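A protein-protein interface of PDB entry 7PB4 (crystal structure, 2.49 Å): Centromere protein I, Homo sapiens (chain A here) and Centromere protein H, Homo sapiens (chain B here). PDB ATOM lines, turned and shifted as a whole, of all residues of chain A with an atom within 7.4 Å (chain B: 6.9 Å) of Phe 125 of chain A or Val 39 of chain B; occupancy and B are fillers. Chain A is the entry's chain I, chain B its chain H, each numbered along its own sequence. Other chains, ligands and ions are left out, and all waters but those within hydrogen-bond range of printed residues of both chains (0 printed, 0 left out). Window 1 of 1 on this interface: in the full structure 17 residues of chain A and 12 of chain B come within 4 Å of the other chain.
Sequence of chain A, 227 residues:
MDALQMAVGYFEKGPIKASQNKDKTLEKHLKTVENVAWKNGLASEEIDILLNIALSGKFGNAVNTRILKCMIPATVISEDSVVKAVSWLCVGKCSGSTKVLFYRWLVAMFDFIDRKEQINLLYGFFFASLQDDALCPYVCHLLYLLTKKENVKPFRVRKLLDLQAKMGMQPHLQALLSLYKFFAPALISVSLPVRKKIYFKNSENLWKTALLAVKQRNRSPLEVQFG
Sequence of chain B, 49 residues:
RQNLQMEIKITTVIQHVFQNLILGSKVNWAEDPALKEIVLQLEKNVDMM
The side-chain hydroxyl of Ser 87 of chain A is in hydrogen-bond range of the backbone NH of Trp 29 of chain B, 3.2 Å away. The indole nitrogen (NE1) of Trp 29 of chain B is in hydrogen-bond range of the side-chain sulfur (SG) of Cys 90 of chain A (3.6 Å). The backbone NH of Ala 30 of chain B sits at hydrogen-bond distance from the side-chain hydroxyl of Ser 87 of chain A (3.1 Å). OE2 of Glu 43 of chain B lies within salt-bridge range of NH1 of Arg 156 of chain A.
O of Trp 29 of chain B is in hydrogen-bond range of N of Lys 36 of chain B, at 3.3 Å. O of Val 86 of chain A is in hydrogen-bond range of SG of Cys 90 of chain A, 3.2 Å away. O of Phe 125 of chain A lies within hydrogen-bond range of OG of Ser 129 of chain A, at 3.4 Å.
Trp 29 of chain B touches Val 83 of chain A (CH2 to CG1, 3.6 Å). SG of Cys 90 of chain A touches CD2 of Leu 23 of chain B, at 3.9 Å. O of Leu 40 of chain B touches CD1 of Leu 121 of chain A, 3.5 Å away. O of Leu 121 of chain A touches CB of Glu 43 of chain B, at 3.6 Å. Leu 122 of chain A touches Trp 29 of chain B. CA of Gly 124 of chain A touches OE1 of Gln 19 of chain B, at 3.2 Å. Phe 125 of chain A touches Gln 19 of chain B. Phe 125 of chain A touches Leu 23 of chain B. Trp 29 of chain B touches Phe 125 of chain A (NE1 to CE1, 3.98 Å). Ala 128 of chain A touches Leu 23 of chain B.
Printed residues of chain B within 4 Å of Ser 87 of chain A: Trp 29 (3.2 Å) and Ala 30 (3.1 Å). Of the printed residues of chain B, Cys 90 of chain A touches Leu 23 (3.9 Å) and Trp 29 (3.6 Å). Printed residues of chain B within 4 Å of Phe 125 of chain A: Gln 19 (3.7 Å), Leu 23 (3.7 Å), Trp 29 (3.98 Å) and Val 39 (3.5 Å). Printed residues of chain A within 4 Å of Gln 19 of chain B: Gly 124 (3.2 Å) and Phe 125 (3.7 Å). Pro 33 of chain B touches none of the printed residues of chain A. Val 39 of chain B touches just one residue of chain A: Phe 125 (3.5 Å).
Among the printed residues, 15 pairs touch across the chains.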
ATOM      1  N   VAL A  83     -11.704  -5.313  31.469  1.00  0.00           N
ATOM      2  CA  VAL A  83     -11.203  -6.687  31.465  1.00  0.00           C
ATOM      3  C   VAL A  83     -12.166  -7.597  30.711  1.00  0.00           C
ATOM      4  O   VAL A  83     -11.759  -8.411  29.871  1.00  0.00           O
ATOM      5  CB  VAL A  83     -10.969  -7.180  32.905  1.00  0.00           C
ATOM      6  CG1 VAL A  83     -10.629  -8.662  32.912  1.00  0.00           C
ATOM      7  CG2 VAL A  83      -9.860  -6.376  33.567  1.00  0.00           C
ATOM      8  N   VAL A  86     -11.813  -6.942  27.030  1.00  0.00           N
ATOM      9  CA  VAL A  86     -10.655  -7.619  26.450  1.00  0.00           C
ATOM     10  C   VAL A  86     -10.947  -9.103  26.270  1.00  0.00           C
ATOM     11  O   VAL A  86     -10.546  -9.716  25.272  1.00  0.00           O
ATOM     12  CB  VAL A  86      -9.406  -7.382  27.319  1.00  0.00           C
ATOM     13  CG1 VAL A  86      -8.234  -8.204  26.807  1.00  0.00           C
ATOM     14  CG2 VAL A  86      -9.049  -5.904  27.338  1.00  0.00           C
ATOM     15  N   SER A  87     -11.664  -9.700  27.224  1.00  0.00           N
ATOM     16  CA  SER A  87     -12.068 -11.096  27.069  1.00  0.00           C
ATOM     17  C   SER A  87     -12.981 -11.275  25.861  1.00  0.00           C
ATOM     18  O   SER A  87     -12.822 -12.227  25.086  1.00  0.00           O
ATOM     19  CB  SER A  87     -12.756 -11.588  28.342  1.00  0.00           C
ATOM     20  OG  SER A  87     -13.101 -12.959  28.241  1.00  0.00           O
ATOM     21  N   CYS A  90     -11.001 -11.326  22.888  1.00  0.00           N
ATOM     22  CA  CYS A  90     -10.348 -12.625  22.751  1.00  0.00           C
ATOM     23  C   CYS A  90     -11.305 -13.688  22.228  1.00  0.00           C
ATOM     24  O   CYS A  90     -10.861 -14.677  21.632  1.00  0.00           O
ATOM     25  CB  CYS A  90      -9.761 -13.068  24.090  1.00  0.00           C
ATOM     26  SG  CYS A  90      -8.404 -12.045  24.698  1.00  0.00           S
ATOM     27  N   TYR A 103     -10.321  -0.027  20.383  1.00  0.00           N
ATOM     28  CA  TYR A 103      -8.981   0.419  20.754  1.00  0.00           C
ATOM     29  C   TYR A 103      -8.892   1.942  20.749  1.00  0.00           C
ATOM     30  O   TYR A 103      -8.269   2.539  21.637  1.00  0.00           O
ATOM     31  CB  TYR A 103      -7.937  -0.192  19.821  1.00  0.00           C
ATOM     32  CG  TYR A 103      -7.536  -1.601  20.204  1.00  0.00           C
ATOM     33  CD1 TYR A 103      -6.644  -1.830  21.243  1.00  0.00           C
ATOM     34  CD2 TYR A 103      -8.048  -2.699  19.527  1.00  0.00           C
ATOM     35  CE1 TYR A 103      -6.276  -3.115  21.599  1.00  0.00           C
ATOM     36  CE2 TYR A 103      -7.686  -3.987  19.875  1.00  0.00           C
ATOM     37  CZ  TYR A 103      -6.799  -4.189  20.911  1.00  0.00           C
ATOM     38  OH  TYR A 103      -6.437  -5.470  21.258  1.00  0.00           O
ATOM     39  N   LEU A 121      -2.201  -5.785  33.553  1.00  0.00           N
ATOM     40  CA  LEU A 121      -2.022  -7.231  33.607  1.00  0.00           C
ATOM     41  C   LEU A 121      -2.369  -7.904  32.284  1.00  0.00           C
ATOM     42  O   LEU A 121      -1.899  -9.019  32.027  1.00  0.00           O
ATOM     43  CB  LEU A 121      -2.869  -7.826  34.734  1.00  0.00           C
ATOM     44  CG  LEU A 121      -2.512  -7.390  36.156  1.00  0.00           C
ATOM     45  CD1 LEU A 121      -3.451  -8.026  37.168  1.00  0.00           C
ATOM     46  CD2 LEU A 121      -1.063  -7.726  36.477  1.00  0.00           C
ATOM     47  N   LEU A 122      -3.178  -7.258  31.443  1.00  0.00           N
ATOM     48  CA  LEU A 122      -3.514  -7.766  30.119  1.00  0.00           C
ATOM     49  C   LEU A 122      -2.546  -7.274  29.045  1.00  0.00           C
ATOM     50  O   LEU A 122      -2.911  -7.224  27.859  1.00  0.00           O
ATOM     51  CB  LEU A 122      -4.950  -7.377  29.761  1.00  0.00           C
ATOM     52  CG  LEU A 122      -5.997  -7.723  30.823  1.00  0.00           C
ATOM     53  CD1 LEU A 122      -7.371  -7.217  30.417  1.00  0.00           C
ATOM     54  CD2 LEU A 122      -6.026  -9.223  31.078  1.00  0.00           C
ATOM     55  N   TYR A 123      -1.324  -6.906  29.440  1.00  0.00           N
ATOM     56  CA  TYR A 123      -0.352  -6.400  28.480  1.00  0.00           C
ATOM     57  C   TYR A 123       0.010  -7.455  27.446  1.00  0.00           C
ATOM     58  O   TYR A 123       0.287  -7.117  26.294  1.00  0.00           O
ATOM     59  CB  TYR A 123       0.904  -5.912  29.203  1.00  0.00           C
ATOM     60  CG  TYR A 123       1.793  -5.023  28.359  1.00  0.00           C
ATOM     61  CD1 TYR A 123       2.737  -5.566  27.497  1.00  0.00           C
ATOM     62  CD2 TYR A 123       1.690  -3.639  28.429  1.00  0.00           C
ATOM     63  CE1 TYR A 123       3.551  -4.757  26.725  1.00  0.00           C
ATOM     64  CE2 TYR A 123       2.500  -2.823  27.662  1.00  0.00           C
ATOM     65  CZ  TYR A 123       3.428  -3.387  26.811  1.00  0.00           C
ATOM     66  OH  TYR A 123       4.235  -2.578  26.046  1.00  0.00           O
ATOM     67  N   GLY A 124       0.006  -8.732  27.829  1.00  0.00           N
ATOM     68  CA  GLY A 124       0.291  -9.780  26.862  1.00  0.00           C
ATOM     69  C   GLY A 124      -0.775  -9.885  25.787  1.00  0.00           C
ATOM     70  O   GLY A 124      -0.462 -10.011  24.599  1.00  0.00           O
ATOM     71  N   PHE A 125      -2.048  -9.838  26.190  1.00  0.00           N
ATOM     72  CA  PHE A 125      -3.134  -9.850  25.215  1.00  0.00           C
ATOM     73  C   PHE A 125      -3.083  -8.616  24.325  1.00  0.00           C
ATOM     74  O   PHE A 125      -3.363  -8.695  23.123  1.00  0.00           O
ATOM     75  CB  PHE A 125      -4.484  -9.938  25.927  1.00  0.00           C
ATOM     76  CG  PHE A 125      -4.689 -11.218  26.685  1.00  0.00           C
ATOM     77  CD1 PHE A 125      -5.244 -12.323  26.063  1.00  0.00           C
ATOM     78  CD2 PHE A 125      -4.330 -11.314  28.018  1.00  0.00           C
ATOM     79  CE1 PHE A 125      -5.438 -13.502  26.758  1.00  0.00           C
ATOM     80  CE2 PHE A 125      -4.519 -12.491  28.717  1.00  0.00           C
ATOM     81  CZ  PHE A 125      -5.075 -13.586  28.086  1.00  0.00           C
ATOM     82  N   PHE A 126      -2.727  -7.463  24.897  1.00  0.00           N
ATOM     83  CA  PHE A 126      -2.606  -6.258  24.081  1.00  0.00           C
ATOM     84  C   PHE A 126      -1.446  -6.368  23.096  1.00  0.00           C
ATOM     85  O   PHE A 126      -1.569  -5.964  21.934  1.00  0.00           O
ATOM     86  CB  PHE A 126      -2.441  -5.032  24.978  1.00  0.00           C
ATOM     87  CG  PHE A 126      -3.705  -4.616  25.673  1.00  0.00           C
ATOM     88  CD1 PHE A 126      -4.908  -4.575  24.988  1.00  0.00           C
ATOM     89  CD2 PHE A 126      -3.694  -4.274  27.015  1.00  0.00           C
ATOM     90  CE1 PHE A 126      -6.074  -4.194  25.626  1.00  0.00           C
ATOM     91  CE2 PHE A 126      -4.856  -3.892  27.659  1.00  0.00           C
ATOM     92  CZ  PHE A 126      -6.047  -3.852  26.963  1.00  0.00           C
ATOM     93  N   PHE A 127      -0.318  -6.928  23.538  1.00  0.00           N
ATOM     94  CA  PHE A 127       0.876  -7.006  22.704  1.00  0.00           C
ATOM     95  C   PHE A 127       0.720  -8.029  21.589  1.00  0.00           C
ATOM     96  O   PHE A 127       1.246  -7.828  20.488  1.00  0.00           O
ATOM     97  CB  PHE A 127       2.087  -7.342  23.577  1.00  0.00           C
ATOM     98  CG  PHE A 127       3.403  -7.293  22.852  1.00  0.00           C
ATOM     99  CD1 PHE A 127       4.125  -6.114  22.779  1.00  0.00           C
ATOM    100  CD2 PHE A 127       3.930  -8.432  22.263  1.00  0.00           C
ATOM    101  CE1 PHE A 127       5.340  -6.067  22.121  1.00  0.00           C
ATOM    102  CE2 PHE A 127       5.143  -8.391  21.604  1.00  0.00           C
ATOM    103  CZ  PHE A 127       5.849  -7.206  21.531  1.00  0.00           C
ATOM    104  N   ALA A 128       0.008  -9.129  21.848  1.00  0.00           N
ATOM    105  CA  ALA A 128      -0.187 -10.146  20.822  1.00  0.00           C
ATOM    106  C   ALA A 128      -1.012  -9.647  19.643  1.00  0.00           C
ATOM    107  O   ALA A 128      -1.022 -10.304  18.596  1.00  0.00           O
ATOM    108  CB  ALA A 128      -0.848 -11.384  21.428  1.00  0.00           C
ATOM    109  N   SER A 129      -1.701  -8.515  19.785  1.00  0.00           N
ATOM    110  CA  SER A 129      -2.471  -7.933  18.695  1.00  0.00           C
ATOM    111  C   SER A 129      -1.617  -7.103  17.745  1.00  0.00           C
ATOM    112  O   SER A 129      -2.164  -6.490  16.823  1.00  0.00           O
ATOM    113  CB  SER A 129      -3.607  -7.073  19.255  1.00  0.00           C
ATOM    114  OG  SER A 129      -4.492  -7.853  20.041  1.00  0.00           O
ATOM    115  N   LEU A 130      -0.298  -7.063  17.950  1.00  0.00           N
ATOM    116  CA  LEU A 130       0.581  -6.369  17.019  1.00  0.00           C
ATOM    117  C   LEU A 130       0.755  -7.132  15.713  1.00  0.00           C
ATOM    118  O   LEU A 130       1.142  -6.530  14.706  1.00  0.00           O
ATOM    119  CB  LEU A 130       1.946  -6.123  17.663  1.00  0.00           C
ATOM    120  CG  LEU A 130       1.995  -5.048  18.751  1.00  0.00           C
ATOM    121  CD1 LEU A 130       3.370  -4.994  19.392  1.00  0.00           C
ATOM    122  CD2 LEU A 130       1.626  -3.697  18.169  1.00  0.00           C
ATOM    123  N   VAL A 139      -3.029  -0.345  18.547  1.00  0.00           N
ATOM    124  CA  VAL A 139      -2.439  -1.132  19.627  1.00  0.00           C
ATOM    125  C   VAL A 139      -1.133  -0.499  20.091  1.00  0.00           C
ATOM    126  O   VAL A 139      -0.827  -0.482  21.289  1.00  0.00           O
ATOM    127  CB  VAL A 139      -2.242  -2.592  19.181  1.00  0.00           C
ATOM    128  CG1 VAL A 139      -1.376  -3.339  20.179  1.00  0.00           C
ATOM    129  CG2 VAL A 139      -3.588  -3.284  19.033  1.00  0.00           C
ATOM    130  N   LEU A 143      -0.362   0.765  23.851  1.00  0.00           N
ATOM    131  CA  LEU A 143       0.794   0.294  24.605  1.00  0.00           C
ATOM    132  C   LEU A 143       1.717   1.441  24.995  1.00  0.00           C
ATOM    133  O   LEU A 143       2.390   1.365  26.028  1.00  0.00           O
ATOM    134  CB  LEU A 143       1.560  -0.756  23.800  1.00  0.00           C
ATOM    135  CG  LEU A 143       0.830  -2.075  23.537  1.00  0.00           C
ATOM    136  CD1 LEU A 143       1.719  -3.041  22.770  1.00  0.00           C
ATOM    137  CD2 LEU A 143       0.358  -2.696  24.839  1.00  0.00           C
ATOM    138  N   ARG A 156       9.519  -9.508  24.197  1.00  0.00           N
ATOM    139  CA  ARG A 156       8.724  -8.469  23.553  1.00  0.00           C
ATOM    140  C   ARG A 156       9.604  -7.497  22.778  1.00  0.00           C
ATOM    141  O   ARG A 156       9.223  -7.044  21.694  1.00  0.00           O
ATOM    142  CB  ARG A 156       7.888  -7.732  24.596  1.00  0.00           C
ATOM    143  CG  ARG A 156       6.770  -8.580  25.161  1.00  0.00           C
ATOM    144  CD  ARG A 156       6.159  -7.956  26.395  1.00  0.00           C
ATOM    145  NE  ARG A 156       4.986  -8.701  26.833  1.00  0.00           N
ATOM    146  CZ  ARG A 156       4.373  -8.515  27.996  1.00  0.00           C
ATOM    147  NH1 ARG A 156       4.827  -7.607  28.849  1.00  0.00           N
ATOM    148  NH2 ARG A 156       3.309  -9.241  28.306  1.00  0.00           N
ATOM    149  N   PHE B  18       0.969 -20.694  28.382  1.00  0.00           N
ATOM    150  CA  PHE B  18      -0.401 -20.621  28.876  1.00  0.00           C
ATOM    151  C   PHE B  18      -1.150 -19.459  28.238  1.00  0.00           C
ATOM    152  O   PHE B  18      -2.307 -19.609  27.823  1.00  0.00           O
ATOM    153  CB  PHE B  18      -0.395 -20.487  30.401  1.00  0.00           C
ATOM    154  CG  PHE B  18      -1.661 -20.956  31.065  1.00  0.00           C
ATOM    155  CD1 PHE B  18      -2.751 -21.369  30.316  1.00  0.00           C
ATOM    156  CD2 PHE B  18      -1.760 -20.979  32.446  1.00  0.00           C
ATOM    157  CE1 PHE B  18      -3.913 -21.799  30.930  1.00  0.00           C
ATOM    158  CE2 PHE B  18      -2.919 -21.407  33.068  1.00  0.00           C
ATOM    159  CZ  PHE B  18      -3.997 -21.817  32.308  1.00  0.00           C
ATOM    160  N   GLN B  19      -0.506 -18.293  28.142  1.00  0.00           N
ATOM    161  CA  GLN B  19      -1.177 -17.138  27.553  1.00  0.00           C
ATOM    162  C   GLN B  19      -1.506 -17.377  26.083  1.00  0.00           C
ATOM    163  O   GLN B  19      -2.617 -17.069  25.629  1.00  0.00           O
ATOM    164  CB  GLN B  19      -0.310 -15.890  27.715  1.00  0.00           C
ATOM    165  CG  GLN B  19      -1.028 -14.597  27.375  1.00  0.00           C
ATOM    166  CD  GLN B  19      -0.196 -13.374  27.696  1.00  0.00           C
ATOM    167  OE1 GLN B  19      -0.667 -12.444  28.351  1.00  0.00           O
ATOM    168  NE2 GLN B  19       1.049 -13.368  27.235  1.00  0.00           N
ATOM    169  N   ASN B  20      -0.560 -17.941  25.327  1.00  0.00           N
ATOM    170  CA  ASN B  20      -0.811 -18.193  23.911  1.00  0.00           C
ATOM    171  C   ASN B  20      -1.891 -19.250  23.715  1.00  0.00           C
ATOM    172  O   ASN B  20      -2.696 -19.152  22.783  1.00  0.00           O
ATOM    173  CB  ASN B  20       0.482 -18.606  23.209  1.00  0.00           C
ATOM    174  CG  ASN B  20       1.469 -17.464  23.093  1.00  0.00           C
ATOM    175  OD1 ASN B  20       1.112 -16.300  23.277  1.00  0.00           O
ATOM    176  ND2 ASN B  20       2.717 -17.789  22.777  1.00  0.00           N
ATOM    177  N   ILE B  22      -4.429 -19.832  25.832  1.00  0.00           N
ATOM    178  CA  ILE B  22      -5.690 -19.172  26.158  1.00  0.00           C
ATOM    179  C   ILE B  22      -6.147 -18.296  25.000  1.00  0.00           C
ATOM    180  O   ILE B  22      -7.342 -18.230  24.683  1.00  0.00           O
ATOM    181  CB  ILE B  22      -5.551 -18.363  27.463  1.00  0.00           C
ATOM    182  CG1 ILE B  22      -5.328 -19.300  28.651  1.00  0.00           C
ATOM    183  CG2 ILE B  22      -6.783 -17.502  27.699  1.00  0.00           C
ATOM    184  CD1 ILE B  22      -5.111 -18.577  29.961  1.00  0.00           C
ATOM    185  N   LEU B  23      -5.204 -17.618  24.340  1.00  0.00           N
ATOM    186  CA  LEU B  23      -5.568 -16.792  23.192  1.00  0.00           C
ATOM    187  C   LEU B  23      -6.029 -17.644  22.013  1.00  0.00           C
ATOM    188  O   LEU B  23      -6.981 -17.280  21.314  1.00  0.00           O
ATOM    189  CB  LEU B  23      -4.391 -15.909  22.786  1.00  0.00           C
ATOM    190  CG  LEU B  23      -4.565 -14.420  23.082  1.00  0.00           C
ATOM    191  CD1 LEU B  23      -3.328 -13.654  22.665  1.00  0.00           C
ATOM    192  CD2 LEU B  23      -5.798 -13.880  22.376  1.00  0.00           C
ATOM    193  N   TRP B  29     -12.538 -16.038  28.859  1.00  0.00           N
ATOM    194  CA  TRP B  29     -11.942 -16.400  30.140  1.00  0.00           C
ATOM    195  C   TRP B  29     -12.476 -15.571  31.300  1.00  0.00           C
ATOM    196  O   TRP B  29     -12.315 -15.976  32.456  1.00  0.00           O
ATOM    197  CB  TRP B  29     -10.419 -16.274  30.062  1.00  0.00           C
ATOM    198  CG  TRP B  29      -9.952 -15.007  29.417  1.00  0.00           C
ATOM    199  CD1 TRP B  29      -9.650 -14.821  28.098  1.00  0.00           C
ATOM    200  CD2 TRP B  29      -9.731 -13.747  30.061  1.00  0.00           C
ATOM    201  NE1 TRP B  29      -9.255 -13.523  27.883  1.00  0.00           N
ATOM    202  CE2 TRP B  29      -9.296 -12.843  29.070  1.00  0.00           C
ATOM    203  CE3 TRP B  29      -9.858 -13.295  31.378  1.00  0.00           C
ATOM    204  CZ2 TRP B  29      -8.989 -11.515  29.357  1.00  0.00           C
ATOM    205  CZ3 TRP B  29      -9.552 -11.977  31.659  1.00  0.00           C
ATOM    206  CH2 TRP B  29      -9.123 -11.102  30.654  1.00  0.00           C
ATOM    207  N   ALA B  30     -13.103 -14.425  31.028  1.00  0.00           N
ATOM    208  CA  ALA B  30     -13.719 -13.658  32.105  1.00  0.00           C
ATOM    209  C   ALA B  30     -14.954 -14.348  32.667  1.00  0.00           C
ATOM    210  O   ALA B  30     -15.323 -14.090  33.817  1.00  0.00           O
ATOM    211  CB  ALA B  30     -14.080 -12.254  31.620  1.00  0.00           C
ATOM    212  N   PRO B  33     -14.448 -18.013  36.476  1.00  0.00           N
ATOM    213  CA  PRO B  33     -13.799 -17.258  37.567  1.00  0.00           C
ATOM    214  C   PRO B  33     -12.356 -17.669  37.812  1.00  0.00           C
ATOM    215  O   PRO B  33     -11.482 -16.802  37.967  1.00  0.00           O
ATOM    216  CB  PRO B  33     -14.697 -17.562  38.777  1.00  0.00           C
ATOM    217  CG  PRO B  33     -16.003 -17.999  38.195  1.00  0.00           C
ATOM    218  CD  PRO B  33     -15.658 -18.717  36.929  1.00  0.00           C
ATOM    219  N   ALA B  34     -12.083 -18.974  37.861  1.00  0.00           N
ATOM    220  CA  ALA B  34     -10.715 -19.435  38.070  1.00  0.00           C
ATOM    221  C   ALA B  34      -9.815 -19.008  36.918  1.00  0.00           C
ATOM    222  O   ALA B  34      -8.710 -18.498  37.134  1.00  0.00           O
ATOM    223  CB  ALA B  34     -10.694 -20.954  38.244  1.00  0.00           C
ATOM    224  N   LEU B  35     -10.280 -19.204  35.681  1.00  0.00           N
ATOM    225  CA  LEU B  35      -9.502 -18.773  34.525  1.00  0.00           C
ATOM    226  C   LEU B  35      -9.258 -17.270  34.553  1.00  0.00           C
ATOM    227  O   LEU B  35      -8.187 -16.802  34.154  1.00  0.00           O
ATOM    228  CB  LEU B  35     -10.210 -19.174  33.232  1.00  0.00           C
ATOM    229  CG  LEU B  35      -9.519 -20.235  32.377  1.00  0.00           C
ATOM    230  CD1 LEU B  35     -10.305 -20.476  31.097  1.00  0.00           C
ATOM    231  CD2 LEU B  35      -8.091 -19.819  32.067  1.00  0.00           C
ATOM    232  N   LYS B  36     -10.237 -16.499  35.029  1.00  0.00           N
ATOM    233  CA  LYS B  36     -10.068 -15.051  35.094  1.00  0.00           C
ATOM    234  C   LYS B  36      -9.016 -14.666  36.126  1.00  0.00           C
ATOM    235  O   LYS B  36      -8.147 -13.828  35.858  1.00  0.00           O
ATOM    236  CB  LYS B  36     -11.402 -14.373  35.406  1.00  0.00           C
ATOM    237  CG  LYS B  36     -11.311 -12.856  35.470  1.00  0.00           C
ATOM    238  CD  LYS B  36     -12.659 -12.224  35.773  1.00  0.00           C
ATOM    239  CE  LYS B  36     -12.557 -10.706  35.799  1.00  0.00           C
ATOM    240  NZ  LYS B  36     -13.864 -10.063  36.108  1.00  0.00           N
ATOM    241  N   GLU B  37      -9.076 -15.269  37.317  1.00  0.00           N
ATOM    242  CA  GLU B  37      -8.099 -14.932  38.346  1.00  0.00           C
ATOM    243  C   GLU B  37      -6.714 -15.487  38.033  1.00  0.00           C
ATOM    244  O   GLU B  37      -5.731 -15.021  38.618  1.00  0.00           O
ATOM    245  CB  GLU B  37      -8.568 -15.425  39.717  1.00  0.00           C
ATOM    246  CG  GLU B  37      -8.633 -16.934  39.867  1.00  0.00           C
ATOM    247  CD  GLU B  37      -9.036 -17.361  41.265  1.00  0.00           C
ATOM    248  OE1 GLU B  37      -8.988 -16.517  42.183  1.00  0.00           O
ATOM    249  OE2 GLU B  37      -9.404 -18.542  41.446  1.00  0.00           O
ATOM    250  N   ILE B  38      -6.614 -16.461  37.132  1.00  0.00           N
ATOM    251  CA  ILE B  38      -5.311 -16.979  36.720  1.00  0.00           C
ATOM    252  C   ILE B  38      -4.726 -16.166  35.570  1.00  0.00           C
ATOM    253  O   ILE B  38      -3.509 -15.975  35.494  1.00  0.00           O
ATOM    254  CB  ILE B  38      -5.441 -18.472  36.355  1.00  0.00           C
ATOM    255  CG1 ILE B  38      -5.751 -19.291  37.608  1.00  0.00           C
ATOM    256  CG2 ILE B  38      -4.172 -18.988  35.692  1.00  0.00           C
ATOM    257  CD1 ILE B  38      -6.433 -20.600  37.313  1.00  0.00           C
ATOM    258  N   VAL B  39      -5.577 -15.676  34.664  1.00  0.00           N
ATOM    259  CA  VAL B  39      -5.103 -14.808  33.588  1.00  0.00           C
ATOM    260  C   VAL B  39      -4.433 -13.568  34.164  1.00  0.00           C
ATOM    261  O   VAL B  39      -3.399 -13.108  33.662  1.00  0.00           O
ATOM    262  CB  VAL B  39      -6.268 -14.448  32.645  1.00  0.00           C
ATOM    263  CG1 VAL B  39      -5.955 -13.188  31.855  1.00  0.00           C
ATOM    264  CG2 VAL B  39      -6.561 -15.606  31.703  1.00  0.00           C
ATOM    265  N   LEU B  40      -4.998 -13.021  35.243  1.00  0.00           N
ATOM    266  CA  LEU B  40      -4.384 -11.882  35.915  1.00  0.00           C
ATOM    267  C   LEU B  40      -3.122 -12.267  36.679  1.00  0.00           C
ATOM    268  O   LEU B  40      -2.345 -11.379  37.047  1.00  0.00           O
ATOM    269  CB  LEU B  40      -5.397 -11.230  36.858  1.00  0.00           C
ATOM    270  CG  LEU B  40      -6.698 -10.781  36.187  1.00  0.00           C
ATOM    271  CD1 LEU B  40      -7.682 -10.232  37.208  1.00  0.00           C
ATOM    272  CD2 LEU B  40      -6.412  -9.751  35.104  1.00  0.00           C
ATOM    273  N   GLN B  41      -2.904 -13.561  36.931  1.00  0.00           N
ATOM    274  CA  GLN B  41      -1.649 -13.991  37.540  1.00  0.00           C
ATOM    275  C   GLN B  41      -0.499 -13.941  36.543  1.00  0.00           C
ATOM    276  O   GLN B  41       0.660 -13.777  36.941  1.00  0.00           O
ATOM    277  CB  GLN B  41      -1.786 -15.403  38.110  1.00  0.00           C
ATOM    278  CG  GLN B  41      -2.692 -15.503  39.323  1.00  0.00           C
ATOM    279  CD  GLN B  41      -2.114 -14.819  40.545  1.00  0.00           C
ATOM    280  OE1 GLN B  41      -0.896 -14.745  40.712  1.00  0.00           O
ATOM    281  NE2 GLN B  41      -2.987 -14.313  41.407  1.00  0.00           N
ATOM    282  N   LEU B  42      -0.794 -14.081  35.255  1.00  0.00           N
ATOM    283  CA  LEU B  42       0.228 -13.940  34.232  1.00  0.00           C
ATOM    284  C   LEU B  42       0.725 -12.495  34.180  1.00  0.00           C
ATOM    285  O   LEU B  42       0.200 -11.602  34.853  1.00  0.00           O
ATOM    286  CB  LEU B  42      -0.315 -14.375  32.872  1.00  0.00           C
ATOM    287  CG  LEU B  42      -0.804 -15.823  32.788  1.00  0.00           C
ATOM    288  CD1 LEU B  42      -1.434 -16.100  31.434  1.00  0.00           C
ATOM    289  CD2 LEU B  42       0.335 -16.792  33.060  1.00  0.00           C
ATOM    290  N   GLU B  43       1.753 -12.273  33.359  1.00  0.00           N
ATOM    291  CA  GLU B  43       2.425 -10.974  33.268  1.00  0.00           C
ATOM    292  C   GLU B  43       2.998 -10.566  34.625  1.00  0.00           C
ATOM    293  O   GLU B  43       2.885  -9.417  35.058  1.00  0.00           O
ATOM    294  CB  GLU B  43       1.488  -9.900  32.700  1.00  0.00           C
ATOM    295  CG  GLU B  43       2.162  -8.587  32.291  1.00  0.00           C
ATOM    296  CD  GLU B  43       3.378  -8.789  31.405  1.00  0.00           C
ATOM    297  OE1 GLU B  43       3.374  -9.729  30.582  1.00  0.00           O
ATOM    298  OE2 GLU B  43       4.341  -8.004  31.535  1.00  0.00           O
